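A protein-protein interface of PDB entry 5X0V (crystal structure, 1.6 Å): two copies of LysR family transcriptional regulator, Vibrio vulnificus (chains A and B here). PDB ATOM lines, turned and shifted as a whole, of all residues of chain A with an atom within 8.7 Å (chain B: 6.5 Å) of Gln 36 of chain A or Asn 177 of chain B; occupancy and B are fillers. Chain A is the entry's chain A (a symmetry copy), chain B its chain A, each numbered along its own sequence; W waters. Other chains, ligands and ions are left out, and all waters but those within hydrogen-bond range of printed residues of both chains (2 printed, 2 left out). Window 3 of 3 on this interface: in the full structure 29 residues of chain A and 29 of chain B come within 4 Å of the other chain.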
ATOM      1  N   LEU A  30       0.938 -11.596  29.123  1.00  0.00           N
ATOM      2  CA  LEU A  30       0.360 -10.425  29.767  1.00  0.00           C
ATOM      3  C   LEU A  30       1.335  -9.247  29.768  1.00  0.00           C
ATOM      4  O   LEU A  30       0.908  -8.089  29.672  1.00  0.00           O
ATOM      5  CB  LEU A  30      -0.052 -10.797  31.211  1.00  0.00           C
ATOM      6  CG  LEU A  30      -0.406  -9.646  32.161  1.00  0.00           C
ATOM      7  CD1 LEU A  30      -1.612  -8.959  31.643  1.00  0.00           C
ATOM      8  CD2 LEU A  30      -0.708 -10.164  33.573  1.00  0.00           C
ATOM      9  N   LEU A  31       2.649  -9.504  29.904  1.00  0.00           N
ATOM     10  CA  LEU A  31       3.583  -8.379  30.062  1.00  0.00           C
ATOM     11  C   LEU A  31       3.743  -7.595  28.771  1.00  0.00           C
ATOM     12  O   LEU A  31       4.077  -6.421  28.843  1.00  0.00           O
ATOM     13  CB  LEU A  31       4.978  -8.828  30.545  1.00  0.00           C
ATOM     14  CG  LEU A  31       4.993  -9.476  31.952  1.00  0.00           C
ATOM     15  CD1 LEU A  31       6.417  -9.967  32.314  1.00  0.00           C
ATOM     16  CD2 LEU A  31       4.502  -8.497  32.993  1.00  0.00           C
ATOM     17  N   CYS A  32       3.498  -8.209  27.604  1.00  0.00           N
ATOM     18  CA  CYS A  32       3.480  -7.424  26.374  1.00  0.00           C
ATOM     19  C   CYS A  32       2.440  -6.326  26.472  1.00  0.00           C
ATOM     20  O   CYS A  32       2.712  -5.177  26.105  1.00  0.00           O
ATOM     21  CB  CYS A  32       3.154  -8.277  25.156  1.00  0.00           C
ATOM     22  SG  CYS A  32       4.327  -9.635  24.843  1.00  0.00           S
ATOM     23  N   ASP A  33       1.224  -6.681  26.914  1.00  0.00           N
ATOM     24  CA  ASP A  33       0.150  -5.691  27.028  1.00  0.00           C
ATOM     25  C   ASP A  33       0.470  -4.666  28.112  1.00  0.00           C
ATOM     26  O   ASP A  33       0.173  -3.470  27.960  1.00  0.00           O
ATOM     27  CB  ASP A  33      -1.182  -6.371  27.399  1.00  0.00           C
ATOM     28  CG  ASP A  33      -1.596  -7.478  26.427  1.00  0.00           C
ATOM     29  OD1 ASP A  33      -1.365  -7.300  25.219  1.00  0.00           O
ATOM     30  OD2 ASP A  33      -2.175  -8.484  26.903  1.00  0.00           O
ATOM     31  N   LEU A  34       1.028  -5.124  29.247  1.00  0.00           N
ATOM     32  CA  LEU A  34       1.338  -4.203  30.340  1.00  0.00           C
ATOM     33  C   LEU A  34       2.353  -3.150  29.910  1.00  0.00           C
ATOM     34  O   LEU A  34       2.173  -1.961  30.193  1.00  0.00           O
ATOM     35  CB  LEU A  34       1.852  -4.971  31.551  1.00  0.00           C
ATOM     36  CG  LEU A  34       2.308  -4.127  32.775  1.00  0.00           C
ATOM     37  CD1 LEU A  34       1.143  -3.376  33.311  1.00  0.00           C
ATOM     38  CD2 LEU A  34       2.874  -5.055  33.844  1.00  0.00           C
ATOM     39  N   VAL A  35       3.390  -3.561  29.157  1.00  0.00           N
ATOM     40  CA  VAL A  35       4.398  -2.605  28.699  1.00  0.00           C
ATOM     41  C   VAL A  35       3.761  -1.553  27.806  1.00  0.00           C
ATOM     42  O   VAL A  35       4.046  -0.351  27.936  1.00  0.00           O
ATOM     43  CB  VAL A  35       5.573  -3.340  28.022  1.00  0.00           C
ATOM     44  CG1 VAL A  35       6.491  -2.348  27.186  1.00  0.00           C
ATOM     45  CG2 VAL A  35       6.425  -3.991  29.120  1.00  0.00           C
ATOM     46  N   GLN A  36       2.933  -1.981  26.843  1.00  0.00           N
ATOM     47  CA  GLN A  36       2.319  -0.987  25.974  1.00  0.00           C
ATOM     48  C   GLN A  36       1.441   0.004  26.746  1.00  0.00           C
ATOM     49  O   GLN A  36       1.474   1.202  26.461  1.00  0.00           O
ATOM     50  CB  GLN A  36       1.507  -1.627  24.854  1.00  0.00           C
ATOM     51  CG  GLN A  36       2.373  -2.464  23.922  1.00  0.00           C
ATOM     52  CD  GLN A  36       3.484  -1.650  23.294  1.00  0.00           C
ATOM     53  OE1 GLN A  36       3.230  -0.614  22.620  1.00  0.00           O
ATOM     54  NE2 GLN A  36       4.752  -2.113  23.489  1.00  0.00           N
ATOM     55  N   GLU A  37       0.682  -0.461  27.741  1.00  0.00           N
ATOM     56  CA  GLU A  37      -0.127   0.464  28.545  1.00  0.00           C
ATOM     57  C   GLU A  37       0.743   1.413  29.362  1.00  0.00           C
ATOM     58  O   GLU A  37       0.488   2.617  29.374  1.00  0.00           O
ATOM     59  CB  GLU A  37      -1.058  -0.292  29.513  1.00  0.00           C
ATOM     60  CG  GLU A  37      -2.175  -1.072  28.841  1.00  0.00           C
ATOM     61  CD  GLU A  37      -2.978  -0.222  27.877  1.00  0.00           C
ATOM     62  OE1 GLU A  37      -3.245   0.957  28.194  1.00  0.00           O
ATOM     63  OE2 GLU A  37      -3.304  -0.744  26.797  1.00  0.00           O
ATOM     64  N   ILE A  38       1.784   0.905  30.028  1.00  0.00           N
ATOM     65  CA  ILE A  38       2.536   1.847  30.881  1.00  0.00           C
ATOM     66  C   ILE A  38       3.388   2.796  30.057  1.00  0.00           C
ATOM     67  O   ILE A  38       3.663   3.920  30.514  1.00  0.00           O
ATOM     68  CB  ILE A  38       3.378   1.122  31.944  1.00  0.00           C
ATOM     69  CG1 ILE A  38       4.401   0.211  31.332  1.00  0.00           C
ATOM     70  CG2 ILE A  38       2.460   0.353  32.970  1.00  0.00           C
ATOM     71  CD1 ILE A  38       5.433  -0.220  32.394  1.00  0.00           C
ATOM     72  N   ASN A  39       3.816   2.406  28.834  1.00  0.00           N
ATOM     73  CA  ASN A  39       4.560   3.345  27.998  1.00  0.00           C
ATOM     74  C   ASN A  39       3.760   4.625  27.803  1.00  0.00           C
ATOM     75  O   ASN A  39       4.305   5.732  27.752  1.00  0.00           O
ATOM     76  CB  ASN A  39       4.826   2.745  26.612  1.00  0.00           C
ATOM     77  CG  ASN A  39       5.984   1.790  26.605  1.00  0.00           C
ATOM     78  OD1 ASN A  39       6.739   1.697  27.578  1.00  0.00           O
ATOM     79  ND2 ASN A  39       6.118   1.052  25.512  1.00  0.00           N
ATOM     80  N   GLN A  40       2.453   4.479  27.656  1.00  0.00           N
ATOM     81  CA  GLN A  40       1.622   5.644  27.447  1.00  0.00           C
ATOM     82  C   GLN A  40       1.197   6.242  28.770  1.00  0.00           C
ATOM     83  O   GLN A  40       1.319   7.450  28.965  1.00  0.00           O
ATOM     84  CB  GLN A  40       0.411   5.254  26.614  1.00  0.00           C
ATOM     85  CG  GLN A  40      -0.557   6.427  26.354  1.00  0.00           C
ATOM     86  CD  GLN A  40      -1.712   6.007  25.504  1.00  0.00           C
ATOM     87  OE1 GLN A  40      -2.573   5.227  25.938  1.00  0.00           O
ATOM     88  NE2 GLN A  40      -1.750   6.514  24.267  1.00  0.00           N
ATOM     89  N   ARG A  41       0.738   5.418  29.706  1.00  0.00           N
ATOM     90  CA  ARG A  41       0.082   5.988  30.863  1.00  0.00           C
ATOM     91  C   ARG A  41       1.053   6.425  31.932  1.00  0.00           C
ATOM     92  O   ARG A  41       0.761   7.361  32.682  1.00  0.00           O
ATOM     93  CB  ARG A  41      -0.929   5.004  31.418  1.00  0.00           C
ATOM     94  CG  ARG A  41      -2.174   5.021  30.552  1.00  0.00           C
ATOM     95  CD  ARG A  41      -2.858   3.683  30.575  1.00  0.00           C
ATOM     96  NE  ARG A  41      -3.566   3.452  31.837  1.00  0.00           N
ATOM     97  CZ  ARG A  41      -4.278   2.348  32.055  1.00  0.00           C
ATOM     98  NH1 ARG A  41      -4.341   1.416  31.094  1.00  0.00           N
ATOM     99  NH2 ARG A  41      -4.914   2.172  33.204  1.00  0.00           N
ATOM    100  N   PHE A  42       2.220   5.806  31.995  1.00  0.00           N
ATOM    101  CA  PHE A  42       3.208   6.082  33.038  1.00  0.00           C
ATOM    102  C   PHE A  42       4.555   6.056  32.356  1.00  0.00           C
ATOM    103  O   PHE A  42       5.358   5.133  32.544  1.00  0.00           O
ATOM    104  CB  PHE A  42       3.104   5.054  34.168  1.00  0.00           C
ATOM    105  CG  PHE A  42       1.747   5.030  34.815  1.00  0.00           C
ATOM    106  CD1 PHE A  42       1.342   6.083  35.625  1.00  0.00           C
ATOM    107  CD2 PHE A  42       0.861   3.994  34.576  1.00  0.00           C
ATOM    108  CE1 PHE A  42       0.084   6.089  36.213  1.00  0.00           C
ATOM    109  CE2 PHE A  42      -0.398   3.996  35.166  1.00  0.00           C
ATOM    110  CZ  PHE A  42      -0.779   5.040  35.988  1.00  0.00           C
ATOM    111  N   PRO A  43       4.847   7.079  31.544  1.00  0.00           N
ATOM    112  CA  PRO A  43       6.004   6.987  30.644  1.00  0.00           C
ATOM    113  C   PRO A  43       7.335   7.112  31.359  1.00  0.00           C
ATOM    114  O   PRO A  43       8.353   6.825  30.733  1.00  0.00           O
ATOM    115  CB  PRO A  43       5.773   8.136  29.636  1.00  0.00           C
ATOM    116  CG  PRO A  43       4.855   9.075  30.317  1.00  0.00           C
ATOM    117  CD  PRO A  43       3.993   8.244  31.255  1.00  0.00           C
ATOM    118  N   LEU A  47      10.544  -0.780  33.677  1.00  0.00           N
ATOM    119  CA  LEU A  47      10.269  -2.087  34.252  1.00  0.00           C
ATOM    120  C   LEU A  47      11.431  -3.018  33.940  1.00  0.00           C
ATOM    121  O   LEU A  47      11.572  -3.439  32.788  1.00  0.00           O
ATOM    122  CB  LEU A  47       8.970  -2.661  33.672  1.00  0.00           C
ATOM    123  CG  LEU A  47       7.631  -2.161  34.097  1.00  0.00           C
ATOM    124  CD1 LEU A  47       6.691  -3.304  33.707  1.00  0.00           C
ATOM    125  CD2 LEU A  47       7.551  -1.866  35.587  1.00  0.00           C
ATOM    126  N   ASP A 171      -5.016 -16.071  23.544  1.00  0.00           N
ATOM    127  CA  ASP A 171      -5.290 -14.718  23.053  1.00  0.00           C
ATOM    128  C   ASP A 171      -4.044 -14.055  22.468  1.00  0.00           C
ATOM    129  O   ASP A 171      -4.172 -13.127  21.648  1.00  0.00           O
ATOM    130  CB  ASP A 171      -5.818 -13.840  24.190  1.00  0.00           C
ATOM    131  CG  ASP A 171      -7.208 -14.253  24.655  1.00  0.00           C
ATOM    132  OD1 ASP A 171      -7.895 -15.046  23.968  1.00  0.00           O
ATOM    133  OD2 ASP A 171      -7.610 -13.765  25.738  1.00  0.00           O
ATOM    134  N   HIS A 172      -2.844 -14.481  22.882  1.00  0.00           N
ATOM    135  CA  HIS A 172      -1.599 -13.968  22.343  1.00  0.00           C
ATOM    136  C   HIS A 172      -1.007 -14.848  21.225  1.00  0.00           C
ATOM    137  O   HIS A 172       0.150 -14.648  20.822  1.00  0.00           O
ATOM    138  CB  HIS A 172      -0.623 -13.746  23.509  1.00  0.00           C
ATOM    139  CG  HIS A 172      -0.841 -12.435  24.200  1.00  0.00           C
ATOM    140  ND1 HIS A 172      -0.137 -11.286  23.863  1.00  0.00           N
ATOM    141  CD2 HIS A 172      -1.735 -12.068  25.155  1.00  0.00           C
ATOM    142  CE1 HIS A 172      -0.593 -10.274  24.582  1.00  0.00           C
ATOM    143  NE2 HIS A 172      -1.557 -10.721  25.379  1.00  0.00           N
ATOM    144  N   GLY A 173      -1.804 -15.753  20.639  1.00  0.00           N
ATOM    145  CA  GLY A 173      -1.329 -16.428  19.439  1.00  0.00           C
ATOM    146  C   GLY A 173      -0.491 -17.678  19.644  1.00  0.00           C
ATOM    147  O   GLY A 173       0.096 -18.162  18.662  1.00  0.00           O
ATOM    148  N   VAL A 214      -3.852  -1.352  36.677  1.00  0.00           N
ATOM    149  CA  VAL A 214      -3.555  -1.481  35.245  1.00  0.00           C
ATOM    150  C   VAL A 214      -3.660  -2.936  34.803  1.00  0.00           C
ATOM    151  O   VAL A 214      -4.245  -3.257  33.758  1.00  0.00           O
ATOM    152  CB  VAL A 214      -2.162  -0.915  34.923  1.00  0.00           C
ATOM    153  CG1 VAL A 214      -1.858  -1.184  33.444  1.00  0.00           C
ATOM    154  CG2 VAL A 214      -2.150   0.554  35.225  1.00  0.00           C
ATOM    155  N   LEU A 218      -6.266  -5.517  31.991  1.00  0.00           N
ATOM    156  CA  LEU A 218      -5.760  -6.366  30.923  1.00  0.00           C
ATOM    157  C   LEU A 218      -6.320  -7.770  30.972  1.00  0.00           C
ATOM    158  O   LEU A 218      -6.021  -8.575  30.083  1.00  0.00           O
ATOM    159  CB  LEU A 218      -4.228  -6.457  30.979  1.00  0.00           C
ATOM    160  CG  LEU A 218      -3.561  -5.102  30.884  1.00  0.00           C
ATOM    161  CD1 LEU A 218      -2.048  -5.213  31.078  1.00  0.00           C
ATOM    162  CD2 LEU A 218      -3.908  -4.440  29.569  1.00  0.00           C
ATOM    163  N   HIS B  97       9.503   4.288  19.817  1.00  0.00           N
ATOM    164  CA  HIS B  97       9.580   5.612  20.475  1.00  0.00           C
ATOM    165  C   HIS B  97      10.995   6.034  20.846  1.00  0.00           C
ATOM    166  O   HIS B  97      11.175   7.164  21.296  1.00  0.00           O
ATOM    167  CB  HIS B  97       8.724   5.698  21.736  1.00  0.00           C
ATOM    168  CG  HIS B  97       7.489   4.866  21.693  1.00  0.00           C
ATOM    169  ND1 HIS B  97       7.393   3.648  22.335  1.00  0.00           N
ATOM    170  CD2 HIS B  97       6.299   5.064  21.071  1.00  0.00           C
ATOM    171  CE1 HIS B  97       6.191   3.145  22.126  1.00  0.00           C
ATOM    172  NE2 HIS B  97       5.509   3.975  21.356  1.00  0.00           N
ATOM    173  N   ALA B 157      10.936  -3.068  24.473  1.00  0.00           N
ATOM    174  CA  ALA B 157       9.680  -2.427  24.079  1.00  0.00           C
ATOM    175  C   ALA B 157       9.284  -1.332  25.067  1.00  0.00           C
ATOM    176  O   ALA B 157       8.576  -0.379  24.694  1.00  0.00           O
ATOM    177  CB  ALA B 157       8.542  -3.469  23.977  1.00  0.00           C
ATOM    178  N   ASN B 158       9.712  -1.448  26.334  1.00  0.00           N
ATOM    179  CA  ASN B 158       9.452  -0.410  27.336  1.00  0.00           C
ATOM    180  C   ASN B 158      10.387   0.782  27.150  1.00  0.00           C
ATOM    181  O   ASN B 158      10.270   1.794  27.885  1.00  0.00           O
ATOM    182  CB  ASN B 158       9.598  -1.097  28.729  1.00  0.00           C
ATOM    183  CG  ASN B 158       9.222  -0.201  29.897  1.00  0.00           C
ATOM    184  OD1 ASN B 158       8.189   0.501  29.894  1.00  0.00           O
ATOM    185  ND2 ASN B 158      10.054  -0.214  30.893  1.00  0.00           N
ATOM    186  N   GLY B 173       6.820 -13.975  14.908  1.00  0.00           N
ATOM    187  CA  GLY B 173       5.907 -13.028  15.534  1.00  0.00           C
ATOM    188  C   GLY B 173       6.281 -12.530  16.920  1.00  0.00           C
ATOM    189  O   GLY B 173       5.435 -11.886  17.564  1.00  0.00           O
ATOM    190  N   LEU B 174       7.483 -12.861  17.427  1.00  0.00           N
ATOM    191  CA  LEU B 174       7.861 -12.405  18.765  1.00  0.00           C
ATOM    192  C   LEU B 174       7.665 -10.890  18.955  1.00  0.00           C
ATOM    193  O   LEU B 174       7.320 -10.433  20.065  1.00  0.00           O
ATOM    194  CB  LEU B 174       9.316 -12.805  19.072  1.00  0.00           C
ATOM    195  CG  LEU B 174       9.762 -12.435  20.491  1.00  0.00           C
ATOM    196  CD1 LEU B 174       8.965 -13.197  21.571  1.00  0.00           C
ATOM    197  CD2 LEU B 174      11.269 -12.773  20.639  1.00  0.00           C
ATOM    198  N   LEU B 175       7.904 -10.077  17.904  1.00  0.00           N
ATOM    199  CA  LEU B 175       7.795  -8.626  18.090  1.00  0.00           C
ATOM    200  C   LEU B 175       6.375  -8.094  17.899  1.00  0.00           C
ATOM    201  O   LEU B 175       6.160  -6.857  18.050  1.00  0.00           O
ATOM    202  CB  LEU B 175       8.728  -7.859  17.120  1.00  0.00           C
ATOM    203  CG  LEU B 175      10.115  -8.516  16.971  1.00  0.00           C
ATOM    204  CD1 LEU B 175      10.886  -7.622  16.075  1.00  0.00           C
ATOM    205  CD2 LEU B 175      10.799  -8.665  18.287  1.00  0.00           C
ATOM    206  N   ASP B 176       5.399  -8.968  17.584  1.00  0.00           N
ATOM    207  CA  ASP B 176       4.074  -8.441  17.203  1.00  0.00           C
ATOM    208  C   ASP B 176       3.496  -7.585  18.315  1.00  0.00           C
ATOM    209  O   ASP B 176       3.504  -7.968  19.503  1.00  0.00           O
ATOM    210  CB  ASP B 176       3.063  -9.558  16.911  1.00  0.00           C
ATOM    211  CG  ASP B 176       3.271 -10.215  15.542  1.00  0.00           C
ATOM    212  OD1 ASP B 176       3.982  -9.657  14.683  1.00  0.00           O
ATOM    213  OD2 ASP B 176       2.678 -11.323  15.348  1.00  0.00           O
ATOM    214  N   ASN B 177       2.919  -6.455  17.887  1.00  0.00           N
ATOM    215  CA  ASN B 177       2.177  -5.553  18.751  1.00  0.00           C
ATOM    216  C   ASN B 177       3.033  -4.935  19.834  1.00  0.00           C
ATOM    217  O   ASN B 177       2.490  -4.424  20.848  1.00  0.00           O
ATOM    218  CB  ASN B 177       0.955  -6.276  19.368  1.00  0.00           C
ATOM    219  CG  ASN B 177      -0.064  -6.627  18.315  1.00  0.00           C
ATOM    220  OD1 ASN B 177      -0.359  -5.802  17.488  1.00  0.00           O
ATOM    221  ND2 ASN B 177      -0.593  -7.849  18.330  1.00  0.00           N
ATOM    222  N   GLN B 178       4.369  -4.931  19.662  1.00  0.00           N
ATOM    223  CA  GLN B 178       5.203  -4.322  20.691  1.00  0.00           C
ATOM    224  C   GLN B 178       5.869  -3.050  20.206  1.00  0.00           C
ATOM    225  O   GLN B 178       6.719  -2.515  20.914  1.00  0.00           O
ATOM    226  CB  GLN B 178       6.255  -5.313  21.190  1.00  0.00           C
ATOM    227  CG  GLN B 178       5.541  -6.587  21.763  1.00  0.00           C
ATOM    228  CD  GLN B 178       6.456  -7.358  22.728  1.00  0.00           C
ATOM    229  OE1 GLN B 178       6.985  -8.430  22.396  1.00  0.00           O
ATOM    230  NE2 GLN B 178       6.701  -6.774  23.885  1.00  0.00           N
ATOM    231  N   ASN B 179       5.480  -2.581  19.012  1.00  0.00           N
ATOM    232  CA  ASN B 179       5.933  -1.313  18.421  1.00  0.00           C
ATOM    233  C   ASN B 179       7.462  -1.174  18.456  1.00  0.00           C
ATOM    234  O   ASN B 179       8.029  -0.206  19.001  1.00  0.00           O
ATOM    235  CB  ASN B 179       5.220  -0.136  19.105  1.00  0.00           C
ATOM    236  CG  ASN B 179       5.301   1.118  18.285  1.00  0.00           C
ATOM    237  OD1 ASN B 179       5.518   1.036  17.066  1.00  0.00           O
ATOM    238  ND2 ASN B 179       5.144   2.282  18.923  1.00  0.00           N
ATOM    239  N   LEU B 180       8.122  -2.167  17.846  1.00  0.00           N
ATOM    240  CA  LEU B 180       9.562  -2.250  17.725  1.00  0.00           C
ATOM    241  C   LEU B 180      10.019  -2.029  16.291  1.00  0.00           C
ATOM    242  O   LEU B 180       9.265  -2.205  15.329  1.00  0.00           O
ATOM    243  CB  LEU B 180      10.047  -3.619  18.188  1.00  0.00           C
ATOM    244  CG  LEU B 180       9.676  -3.863  19.656  1.00  0.00           C
ATOM    245  CD1 LEU B 180       9.853  -5.332  19.970  1.00  0.00           C
ATOM    246  CD2 LEU B 180      10.556  -2.997  20.522  1.00  0.00           C
HETATM  247  O   HOH W   1       5.212  -4.656  24.691  1.00  0.00           O
HETATM  248  O   HOH W   2       1.491  -6.090  23.083  1.00  0.00           O
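O of Ala 157 of chain B sits at hydrogen-bond distance from ND2 of Asn 39 of chain A (3.0 Å). The side-chain amide nitrogen of Gln 36 of chain A is in hydrogen-bond range of the backbone carbonyl oxygen of Gln 178 of chain B (3.3 Å). The side-chain amide nitrogen of Asn 158 of chain B sits close to the backbone NH of Leu 47 of chain A (2.9 Å). The side-chain amide oxygen (OD1) of Asn 39 of chain A lies close to the side-chain amide oxygen (OD1) of Asn 158 of chain B, 3.0 Å away.
The backbone carbonyl oxygen of Val 35 of chain A lies close to the side-chain amide oxygen of Asn 39 of chain A (3.4 Å). The backbone carbonyl oxygen of Leu 174 of chain B lies close to the side-chain amide oxygen of Gln 178 of chain B. A ring nitrogen (NE2) of His 97 of chain B sits at hydrogen-bond distance from the side-chain amide nitrogen of Asn 179 of chain B.
CD of Gln 178 of chain B touches SG of Cys 32 of chain A, 3.8 Å away. Ala 157 of chain B touches Val 35 of chain A (C to CG1, 3.7 Å). N of Asn 158 of chain B touches CG1 of Val 35 of chain A, at 3.5 Å. O of Asn 177 of chain B touches CG of Gln 36 of chain A, at 3.6 Å. CD1 of Ile 38 of chain A touches OD1 of Asn 158 of chain B (3.8 Å). ND2 of Asn 39 of chain A touches CE1 of His 97 of chain B, at 3.98 Å.
Of the printed residues of chain B, Val 35 of chain A touches Ala 157 and Asn 158. Of the printed residues of chain B, Gln 36 of chain A touches Asn 177 and Gln 178. Of the printed residues of chain B, Leu 47 of chain A touches Asn 158. Of the printed residues of chain A, Ala 157 of chain B touches Val 35 and Asn 39. Leu 175 of chain B touches none of the printed residues of chain A. Asn 177 of chain B touches one residue of chain A. Of the printed residues of chain A, Gln 178 of chain B touches Cys 32 (3.8 Å) and Gln 36 (3.3 Å). The nearest printed residue of chain B that does not touch Gln 36 of chain A is Ala 157 of chain B (4.1 Å). The nearest residue of chain A that does not touch Asn 177 of chain B is Cys 32 of chain A (5.3 Å).
Printed residues of chain B that touch a printed residue of chain A: His 97, Ala 157, Asn 158, Asn 177 and Gln 178. Hydrophobic or aromatic side chains of chain A within 4 Å of the printed part of chain B: Val 35, Ile 38 and Leu 47. Among the printed residues, 10 pairs touch across the chains.
Position printed for both chains: 173. Of the 10 pairs that touch across the chains among the printed residues, none has its exchanged pair printed and touching as well.
Water W1 lies within hydrogen-bond range of the side-chain amide nitrogen of Gln 178 of chain B (2.7 Å), the side-chain amide nitrogen of Gln 36 of chain A (2.9 Å) and the backbone carbonyl oxygen of Cys 32 of chain A (2.9 Å). Water W2 lies within hydrogen-bond range of O of Asn 177 of chain B (3.0 Å) and O of Cys 32 of chain A (3.4 Å).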
